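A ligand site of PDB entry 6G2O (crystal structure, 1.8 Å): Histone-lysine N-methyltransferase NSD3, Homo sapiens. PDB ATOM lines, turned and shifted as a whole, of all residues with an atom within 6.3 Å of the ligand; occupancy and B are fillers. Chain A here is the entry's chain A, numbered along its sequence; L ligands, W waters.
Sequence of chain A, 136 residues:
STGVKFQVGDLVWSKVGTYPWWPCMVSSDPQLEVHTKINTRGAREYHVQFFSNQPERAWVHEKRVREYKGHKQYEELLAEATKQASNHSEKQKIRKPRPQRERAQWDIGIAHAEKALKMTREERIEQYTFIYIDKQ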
ATOM      1  N   SER A  14      18.319 -16.403  17.420  1.00  0.00           N
ATOM      2  CA  SER A  14      19.138 -16.838  16.274  1.00  0.00           C
ATOM      3  C   SER A  14      20.029 -15.675  15.843  1.00  0.00           C
ATOM      4  O   SER A  14      19.556 -14.532  15.770  1.00  0.00           O
ATOM      5  CB  SER A  14      18.281 -17.281  15.091  1.00  0.00           C
ATOM      6  OG  SER A  14      17.325 -18.264  15.463  1.00  0.00           O
ATOM      7  N   VAL A  16      22.037 -14.505  12.710  1.00  0.00           N
ATOM      8  CA  VAL A  16      22.134 -14.710  11.264  1.00  0.00           C
ATOM      9  C   VAL A  16      22.655 -13.452  10.574  1.00  0.00           C
ATOM     10  O   VAL A  16      22.077 -12.377  10.744  1.00  0.00           O
ATOM     11  CB  VAL A  16      20.767 -15.165  10.651  1.00  0.00           C
ATOM     12  CG1 VAL A  16      20.889 -15.355   9.134  1.00  0.00           C
ATOM     13  CG2 VAL A  16      20.224 -16.417  11.324  1.00  0.00           C
ATOM     14  N   GLY A  17      23.669 -13.628   9.731  1.00  0.00           N
ATOM     15  CA  GLY A  17      24.314 -12.588   8.939  1.00  0.00           C
ATOM     16  C   GLY A  17      24.741 -11.362   9.712  1.00  0.00           C
ATOM     17  O   GLY A  17      25.394 -11.463  10.755  1.00  0.00           O
ATOM     18  N   TYR A  19      22.751  -9.280  11.260  1.00  0.00           N
ATOM     19  CA  TYR A  19      21.685  -8.947  12.199  1.00  0.00           C
ATOM     20  C   TYR A  19      21.954  -9.382  13.645  1.00  0.00           C
ATOM     21  O   TYR A  19      22.611 -10.399  13.882  1.00  0.00           O
ATOM     22  CB  TYR A  19      20.353  -9.508  11.659  1.00  0.00           C
ATOM     23  CG  TYR A  19      20.042  -8.983  10.280  1.00  0.00           C
ATOM     24  CD1 TYR A  19      19.642  -7.653  10.095  1.00  0.00           C
ATOM     25  CD2 TYR A  19      20.262  -9.765   9.148  1.00  0.00           C
ATOM     26  CE1 TYR A  19      19.420  -7.144   8.817  1.00  0.00           C
ATOM     27  CE2 TYR A  19      20.040  -9.256   7.870  1.00  0.00           C
ATOM     28  CZ  TYR A  19      19.608  -7.954   7.705  1.00  0.00           C
ATOM     29  OH  TYR A  19      19.376  -7.454   6.437  1.00  0.00           O
ATOM     30  N   PRO A  20      21.488  -8.590  14.638  1.00  0.00           N
ATOM     31  CA  PRO A  20      21.677  -8.977  16.037  1.00  0.00           C
ATOM     32  C   PRO A  20      20.887 -10.248  16.404  1.00  0.00           C
ATOM     33  O   PRO A  20      20.013 -10.692  15.648  1.00  0.00           O
ATOM     34  CB  PRO A  20      21.139  -7.772  16.819  1.00  0.00           C
ATOM     35  CG  PRO A  20      20.105  -7.189  15.926  1.00  0.00           C
ATOM     36  CD  PRO A  20      20.679  -7.356  14.536  1.00  0.00           C
ATOM     37  N   TRP A  22      18.267 -12.515  17.309  1.00  0.00           N
ATOM     38  CA  TRP A  22      16.854 -12.232  17.025  1.00  0.00           C
ATOM     39  C   TRP A  22      15.905 -13.264  17.612  1.00  0.00           C
ATOM     40  O   TRP A  22      16.167 -14.464  17.482  1.00  0.00           O
ATOM     41  CB  TRP A  22      16.666 -12.144  15.503  1.00  0.00           C
ATOM     42  CG  TRP A  22      15.562 -11.226  15.089  1.00  0.00           C
ATOM     43  CD1 TRP A  22      14.233 -11.525  15.041  1.00  0.00           C
ATOM     44  CD2 TRP A  22      15.681  -9.846  14.673  1.00  0.00           C
ATOM     45  NE1 TRP A  22      13.517 -10.427  14.628  1.00  0.00           N
ATOM     46  CE2 TRP A  22      14.372  -9.386  14.395  1.00  0.00           C
ATOM     47  CE3 TRP A  22      16.766  -8.968  14.509  1.00  0.00           C
ATOM     48  CZ2 TRP A  22      14.116  -8.074  13.962  1.00  0.00           C
ATOM     49  CZ3 TRP A  22      16.517  -7.676  14.062  1.00  0.00           C
ATOM     50  CH2 TRP A  22      15.209  -7.229  13.813  1.00  0.00           C
ATOM     51  N   PHE A  50      11.425 -16.125  12.190  1.00  0.00           N
ATOM     52  CA  PHE A  50      11.806 -14.895  12.906  1.00  0.00           C
ATOM     53  C   PHE A  50      10.546 -14.145  13.333  1.00  0.00           C
ATOM     54  O   PHE A  50       9.669 -13.895  12.492  1.00  0.00           O
ATOM     55  CB  PHE A  50      12.668 -13.985  12.016  1.00  0.00           C
ATOM     56  CG  PHE A  50      14.050 -14.551  11.766  1.00  0.00           C
ATOM     57  CD1 PHE A  50      14.251 -15.570  10.836  1.00  0.00           C
ATOM     58  CD2 PHE A  50      15.145 -14.092  12.485  1.00  0.00           C
ATOM     59  CE1 PHE A  50      15.520 -16.117  10.639  1.00  0.00           C
ATOM     60  CE2 PHE A  50      16.424 -14.617  12.260  1.00  0.00           C
ATOM     61  CZ  PHE A  50      16.597 -15.611  11.326  1.00  0.00           C
ATOM     62  N   PHE A  51      10.479 -13.718  14.605  1.00  0.00           N
ATOM     63  CA  PHE A  51       9.392 -12.870  15.122  1.00  0.00           C
ATOM     64  C   PHE A  51       9.701 -11.458  14.643  1.00  0.00           C
ATOM     65  O   PHE A  51      10.773 -10.911  14.941  1.00  0.00           O
ATOM     66  CB  PHE A  51       9.314 -12.901  16.644  1.00  0.00           C
ATOM     67  CG  PHE A  51       8.685 -14.163  17.171  1.00  0.00           C
ATOM     68  CD1 PHE A  51       7.316 -14.384  17.036  1.00  0.00           C
ATOM     69  CD2 PHE A  51       9.438 -15.106  17.846  1.00  0.00           C
ATOM     70  CE1 PHE A  51       6.712 -15.530  17.577  1.00  0.00           C
ATOM     71  CE2 PHE A  51       8.842 -16.251  18.366  1.00  0.00           C
ATOM     72  CZ  PHE A  51       7.487 -16.454  18.242  1.00  0.00           C
ATOM     73  N   SER A  52       8.798 -10.897  13.858  1.00  0.00           N
ATOM     74  CA  SER A  52       8.977  -9.590  13.234  1.00  0.00           C
ATOM     75  C   SER A  52       7.676  -9.165  12.586  1.00  0.00           C
ATOM     76  O   SER A  52       6.782  -9.992  12.386  1.00  0.00           O
ATOM     77  CB  SER A  52      10.018  -9.735  12.120  1.00  0.00           C
ATOM     78  OG  SER A  52      10.242  -8.554  11.394  1.00  0.00           O
ATOM     79  N   ASN A  53       7.606  -7.898  12.140  1.00  0.00           N
ATOM     80  CA  ASN A  53       6.466  -7.436  11.351  1.00  0.00           C
ATOM     81  C   ASN A  53       6.718  -7.948   9.910  1.00  0.00           C
ATOM     82  O   ASN A  53       5.812  -7.953   9.096  1.00  0.00           O
ATOM     83  CB  ASN A  53       6.329  -5.896  11.396  1.00  0.00           C
ATOM     84  CG  ASN A  53       7.528  -5.168  10.846  1.00  0.00           C
ATOM     85  OD1 ASN A  53       8.673  -5.418  11.249  1.00  0.00           O
ATOM     86  ND2 ASN A  53       7.282  -4.251   9.911  1.00  0.00           N
ATOM     87  N   GLN A  54       7.982  -8.369   9.610  1.00  0.00           N
ATOM     88  CA  GLN A  54       8.290  -8.948   8.306  1.00  0.00           C
ATOM     89  C   GLN A  54       8.631 -10.422   8.486  1.00  0.00           C
ATOM     90  O   GLN A  54       9.752 -10.768   8.867  1.00  0.00           O
ATOM     91  CB  GLN A  54       9.316  -8.137   7.459  1.00  0.00           C
ATOM     92  CG  GLN A  54      10.740  -8.079   7.931  1.00  0.00           C
ATOM     93  CD  GLN A  54      11.644  -7.567   6.850  1.00  0.00           C
ATOM     94  OE1 GLN A  54      12.043  -6.402   6.856  1.00  0.00           O
ATOM     95  NE2 GLN A  54      12.015  -8.423   5.897  1.00  0.00           N
ATOM     96  N   PRO A  55       7.630 -11.309   8.307  1.00  0.00           N
ATOM     97  CA  PRO A  55       7.882 -12.739   8.552  1.00  0.00           C
ATOM     98  C   PRO A  55       8.928 -13.324   7.619  1.00  0.00           C
ATOM     99  O   PRO A  55       8.939 -13.040   6.422  1.00  0.00           O
ATOM    100  CB  PRO A  55       6.490 -13.359   8.384  1.00  0.00           C
ATOM    101  CG  PRO A  55       5.753 -12.430   7.483  1.00  0.00           C
ATOM    102  CD  PRO A  55       6.223 -11.066   7.927  1.00  0.00           C
ATOM    103  N   GLU A  56       9.877 -14.079   8.202  1.00  0.00           N
ATOM    104  CA  GLU A  56      10.976 -14.729   7.478  1.00  0.00           C
ATOM    105  C   GLU A  56      11.299 -16.041   8.159  1.00  0.00           C
ATOM    106  O   GLU A  56      11.029 -16.197   9.356  1.00  0.00           O
ATOM    107  CB  GLU A  56      12.248 -13.853   7.450  1.00  0.00           C
ATOM    108  CG  GLU A  56      12.145 -12.490   6.767  1.00  0.00           C
ATOM    109  CD  GLU A  56      11.825 -12.429   5.283  1.00  0.00           C
ATOM    110  OE1 GLU A  56      11.598 -11.316   4.780  1.00  0.00           O
ATOM    111  OE2 GLU A  56      11.796 -13.490   4.621  1.00  0.00           O
ATOM    112  N   ARG A  57      11.894 -16.974   7.409  1.00  0.00           N
ATOM    113  CA  ARG A  57      12.361 -18.271   7.897  1.00  0.00           C
ATOM    114  C   ARG A  57      13.799 -18.487   7.478  1.00  0.00           C
ATOM    115  O   ARG A  57      14.261 -17.867   6.501  1.00  0.00           O
ATOM    116  CB  ARG A  57      11.463 -19.435   7.387  1.00  0.00           C
ATOM    117  CG  ARG A  57      11.242 -19.433   5.856  1.00  0.00           C
ATOM    118  CD  ARG A  57      10.823 -20.778   5.289  1.00  0.00           C
ATOM    119  NE  ARG A  57      11.985 -21.601   4.982  1.00  0.00           N
ATOM    120  CZ  ARG A  57      12.077 -22.440   3.955  1.00  0.00           C
ATOM    121  NH1 ARG A  57      13.184 -23.137   3.751  1.00  0.00           N
ATOM    122  NH2 ARG A  57      11.049 -22.588   3.121  1.00  0.00           N
ATOM    123  N   ALA A  58      14.533 -19.371   8.183  1.00  0.00           N
ATOM    124  CA  ALA A  58      15.912 -19.721   7.842  1.00  0.00           C
ATOM    125  C   ALA A  58      16.368 -21.010   8.514  1.00  0.00           C
ATOM    126  O   ALA A  58      15.871 -21.355   9.604  1.00  0.00           O
ATOM    127  CB  ALA A  58      16.875 -18.593   8.240  1.00  0.00           C
ATOM    128  N   ARG A 101      15.285   1.726  12.452  1.00  0.00           N
ATOM    129  CA  ARG A 101      14.298   0.879  11.781  1.00  0.00           C
ATOM    130  C   ARG A 101      14.463  -0.592  12.210  1.00  0.00           C
ATOM    131  O   ARG A 101      13.456  -1.262  12.488  1.00  0.00           O
ATOM    132  CB  ARG A 101      14.360   1.106  10.257  1.00  0.00           C
ATOM    133  CG  ARG A 101      14.125  -0.099   9.349  1.00  0.00           C
ATOM    134  CD  ARG A 101      14.555   0.168   7.910  1.00  0.00           C
ATOM    135  NE  ARG A 101      15.998   0.392   7.775  1.00  0.00           N
ATOM    136  CZ  ARG A 101      16.562   1.579   7.588  1.00  0.00           C
ATOM    137  NH1 ARG A 101      15.818   2.670   7.501  1.00  0.00           N
ATOM    138  NH2 ARG A 101      17.883   1.683   7.498  1.00  0.00           N
ATOM    139  N   GLU A 102      15.710  -1.072  12.308  1.00  0.00           N
ATOM    140  CA  GLU A 102      16.013  -2.434  12.761  1.00  0.00           C
ATOM    141  C   GLU A 102      15.594  -2.634  14.228  1.00  0.00           C
ATOM    142  O   GLU A 102      14.974  -3.649  14.556  1.00  0.00           O
ATOM    143  CB  GLU A 102      17.513  -2.749  12.566  1.00  0.00           C
ATOM    144  CG  GLU A 102      17.892  -4.182  12.860  1.00  0.00           C
ATOM    145  CD  GLU A 102      19.375  -4.428  12.707  1.00  0.00           C
ATOM    146  OE1 GLU A 102      19.814  -4.751  11.570  1.00  0.00           O
ATOM    147  OE2 GLU A 102      20.117  -4.261  13.699  1.00  0.00           O
ATOM    148  N   ARG A 103      15.919  -1.651  15.098  1.00  0.00           N
ATOM    149  CA  ARG A 103      15.560  -1.661  16.526  1.00  0.00           C
ATOM    150  C   ARG A 103      14.029  -1.736  16.699  1.00  0.00           C
ATOM    151  O   ARG A 103      13.553  -2.510  17.534  1.00  0.00           O
ATOM    152  CB  ARG A 103      16.173  -0.433  17.242  1.00  0.00           C
ATOM    153  CG  ARG A 103      15.686  -0.171  18.669  1.00  0.00           C
ATOM    154  CD  ARG A 103      16.089  -1.259  19.657  1.00  0.00           C
ATOM    155  NE  ARG A 103      15.596  -0.975  20.997  1.00  0.00           N
ATOM    156  CZ  ARG A 103      15.902  -1.694  22.075  1.00  0.00           C
ATOM    157  NH1 ARG A 103      15.407  -1.370  23.258  1.00  0.00           N
ATOM    158  NH2 ARG A 103      16.702  -2.748  21.970  1.00  0.00           N
ATOM    159  N   GLN A 105      11.773  -2.979  14.532  1.00  0.00           N
ATOM    160  CA  GLN A 105      11.332  -4.313  14.141  1.00  0.00           C
ATOM    161  C   GLN A 105      11.739  -5.350  15.208  1.00  0.00           C
ATOM    162  O   GLN A 105      10.926  -6.215  15.533  1.00  0.00           O
ATOM    163  CB  GLN A 105      11.870  -4.676  12.737  1.00  0.00           C
ATOM    164  CG  GLN A 105      11.344  -3.751  11.635  1.00  0.00           C
ATOM    165  CD  GLN A 105      11.730  -4.196  10.242  1.00  0.00           C
ATOM    166  OE1 GLN A 105      12.702  -3.705   9.648  1.00  0.00           O
ATOM    167  NE2 GLN A 105      10.977  -5.130   9.680  1.00  0.00           N
ATOM    168  N   TRP A 106      12.946  -5.198  15.813  1.00  0.00           N
ATOM    169  CA  TRP A 106      13.434  -6.083  16.884  1.00  0.00           C
ATOM    170  C   TRP A 106      12.508  -6.000  18.111  1.00  0.00           C
ATOM    171  O   TRP A 106      12.088  -7.035  18.621  1.00  0.00           O
ATOM    172  CB  TRP A 106      14.872  -5.750  17.261  1.00  0.00           C
ATOM    173  CG  TRP A 106      15.481  -6.711  18.229  1.00  0.00           C
ATOM    174  CD1 TRP A 106      16.224  -7.825  17.938  1.00  0.00           C
ATOM    175  CD2 TRP A 106      15.527  -6.575  19.663  1.00  0.00           C
ATOM    176  NE1 TRP A 106      16.709  -8.395  19.093  1.00  0.00           N
ATOM    177  CE2 TRP A 106      16.318  -7.634  20.166  1.00  0.00           C
ATOM    178  CE3 TRP A 106      15.042  -5.605  20.560  1.00  0.00           C
ATOM    179  CZ2 TRP A 106      16.583  -7.784  21.531  1.00  0.00           C
ATOM    180  CZ3 TRP A 106      15.284  -5.770  21.915  1.00  0.00           C
ATOM    181  CH2 TRP A 106      16.072  -6.835  22.387  1.00  0.00           C
HETATM  182  C1  LIG L   1      15.190 -12.510   4.422  1.00  0.00           C
HETATM  183  C2  LIG L   1      15.324 -13.604   5.271  1.00  0.00           C
HETATM  184  C3  LIG L   1      15.837 -13.493   6.560  1.00  0.00           C
HETATM  185  C4  LIG L   1      14.630 -12.673   3.039  1.00  0.00           C
HETATM  186  C5  LIG L   1      16.852 -12.072   8.362  1.00  0.00           C
HETATM  187  C6  LIG L   1      16.369 -11.436   9.476  1.00  0.00           C
HETATM  188  C7  LIG L   1      17.349 -11.173  11.860  1.00  0.00           C
HETATM  189  C8  LIG L   1      12.748 -10.756   9.987  1.00  0.00           C
HETATM  190  C9  LIG L   1      13.797  -8.724  10.230  1.00  0.00           C
HETATM  191  C10 LIG L   1      15.078  -9.297   9.988  1.00  0.00           C
HETATM  192  C11 LIG L   1      16.221  -8.441  10.009  1.00  0.00           C
HETATM  193  C12 LIG L   1      14.834  -6.583  10.510  1.00  0.00           C
HETATM  194  C13 LIG L   1      16.257 -12.214   7.006  1.00  0.00           C
HETATM  195  C14 LIG L   1      18.343 -12.362   9.895  1.00  0.00           C
HETATM  196  C15 LIG L   1      15.108 -10.702   9.719  1.00  0.00           C
HETATM  197  C16 LIG L   1      13.933 -11.412   9.701  1.00  0.00           C
HETATM  198  C17 LIG L   1      15.925 -14.723   7.414  1.00  0.00           C
HETATM  199  C18 LIG L   1      16.156 -11.095   6.157  1.00  0.00           C
HETATM  200  C19 LIG L   1      16.092  -7.116  10.296  1.00  0.00           C
HETATM  201  C20 LIG L   1      13.704  -7.329  10.484  1.00  0.00           C
HETATM  202  C21 LIG L   1      16.566  -9.709   6.579  1.00  0.00           C
HETATM  203  C22 LIG L   1      15.607 -11.263   4.884  1.00  0.00           C
HETATM  204  F1  LIG L   1      14.746  -5.266  10.813  1.00  0.00           F
HETATM  205  N1  LIG L   1      18.096 -12.635   8.632  1.00  0.00           N
HETATM  206  N2  LIG L   1      12.641  -9.458  10.218  1.00  0.00           N
HETATM  207  N3  LIG L   1      13.673 -11.599   2.675  1.00  0.00           N
HETATM  208  N4  LIG L   1      17.371 -11.631  10.477  1.00  0.00           N
HETATM  209  O   HOH W   1      19.874 -12.660  13.754  1.00  0.00           O
HETATM  210  O   HOH W   2      19.593 -13.354   6.263  1.00  0.00           O
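OE1 of Glu 56 sits at hydrogen-bond distance from NE2 of Gln 54, at 3.1 Å.
The backbone NH of Phe 50 is in hydrogen-bond range of the backbone carbonyl oxygen of Glu 56 (2.9 Å).
The indole nitrogen of Trp 22 lies within hydrogen-bond range of the backbone carbonyl oxygen of Phe 51.
The side-chain amide nitrogen (NE2) of Gln 105 lies within hydrogen-bond range of the side-chain amide oxygen (OD1) of Asn 53 (2.8 Å).
N of Gln 54 lies within hydrogen-bond range of OG of Ser 52.
N of Trp 22 lies within hydrogen-bond range of O of Ser 14 (2.8 Å).
NE2 of Gln 105 lies within hydrogen-bond range of OE1 of Gln 54.
Water W1 lies within hydrogen-bond range of O of Pro 20 (2.7 Å), O of Ser 14 (2.8 Å) and N of Val 16 (3.0 Å).
The side-chain carboxylate of Glu 56 lies within salt-bridge range of a nitrogen (N3) of the ligand (3.0 Å).
A nitrogen (N2) of the ligand is in hydrogen-bond range of the side-chain hydroxyl of Ser 52.
The backbone carbonyl oxygen (O) of Gln 54 sits close to a nitrogen (N2) of the ligand.
OE1 of Gln 105 lies close to F1 of the ligand (2.8 Å).
Merely in contact with the ligand: Tyr 19, Trp 22, Phe 50, Glu 102, Arg 57 and Val 16.
Hydrophobic or aromatic side chains that line the ligand: Val 16, Tyr 19, Trp 22 and Phe 50.
Ten residues have an atom within 4 Å of the ligand: Val 16, Tyr 19, Trp 22, Phe 50, Ser 52, Gln 54, Glu 56, Arg 57, Glu 102 and Gln 105.
Along chain A the residues within 4 Å of the ligand span positions 16 to 105.
The nearest printed residue that does not touch the ligand is Ala 58 (4.1 Å).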
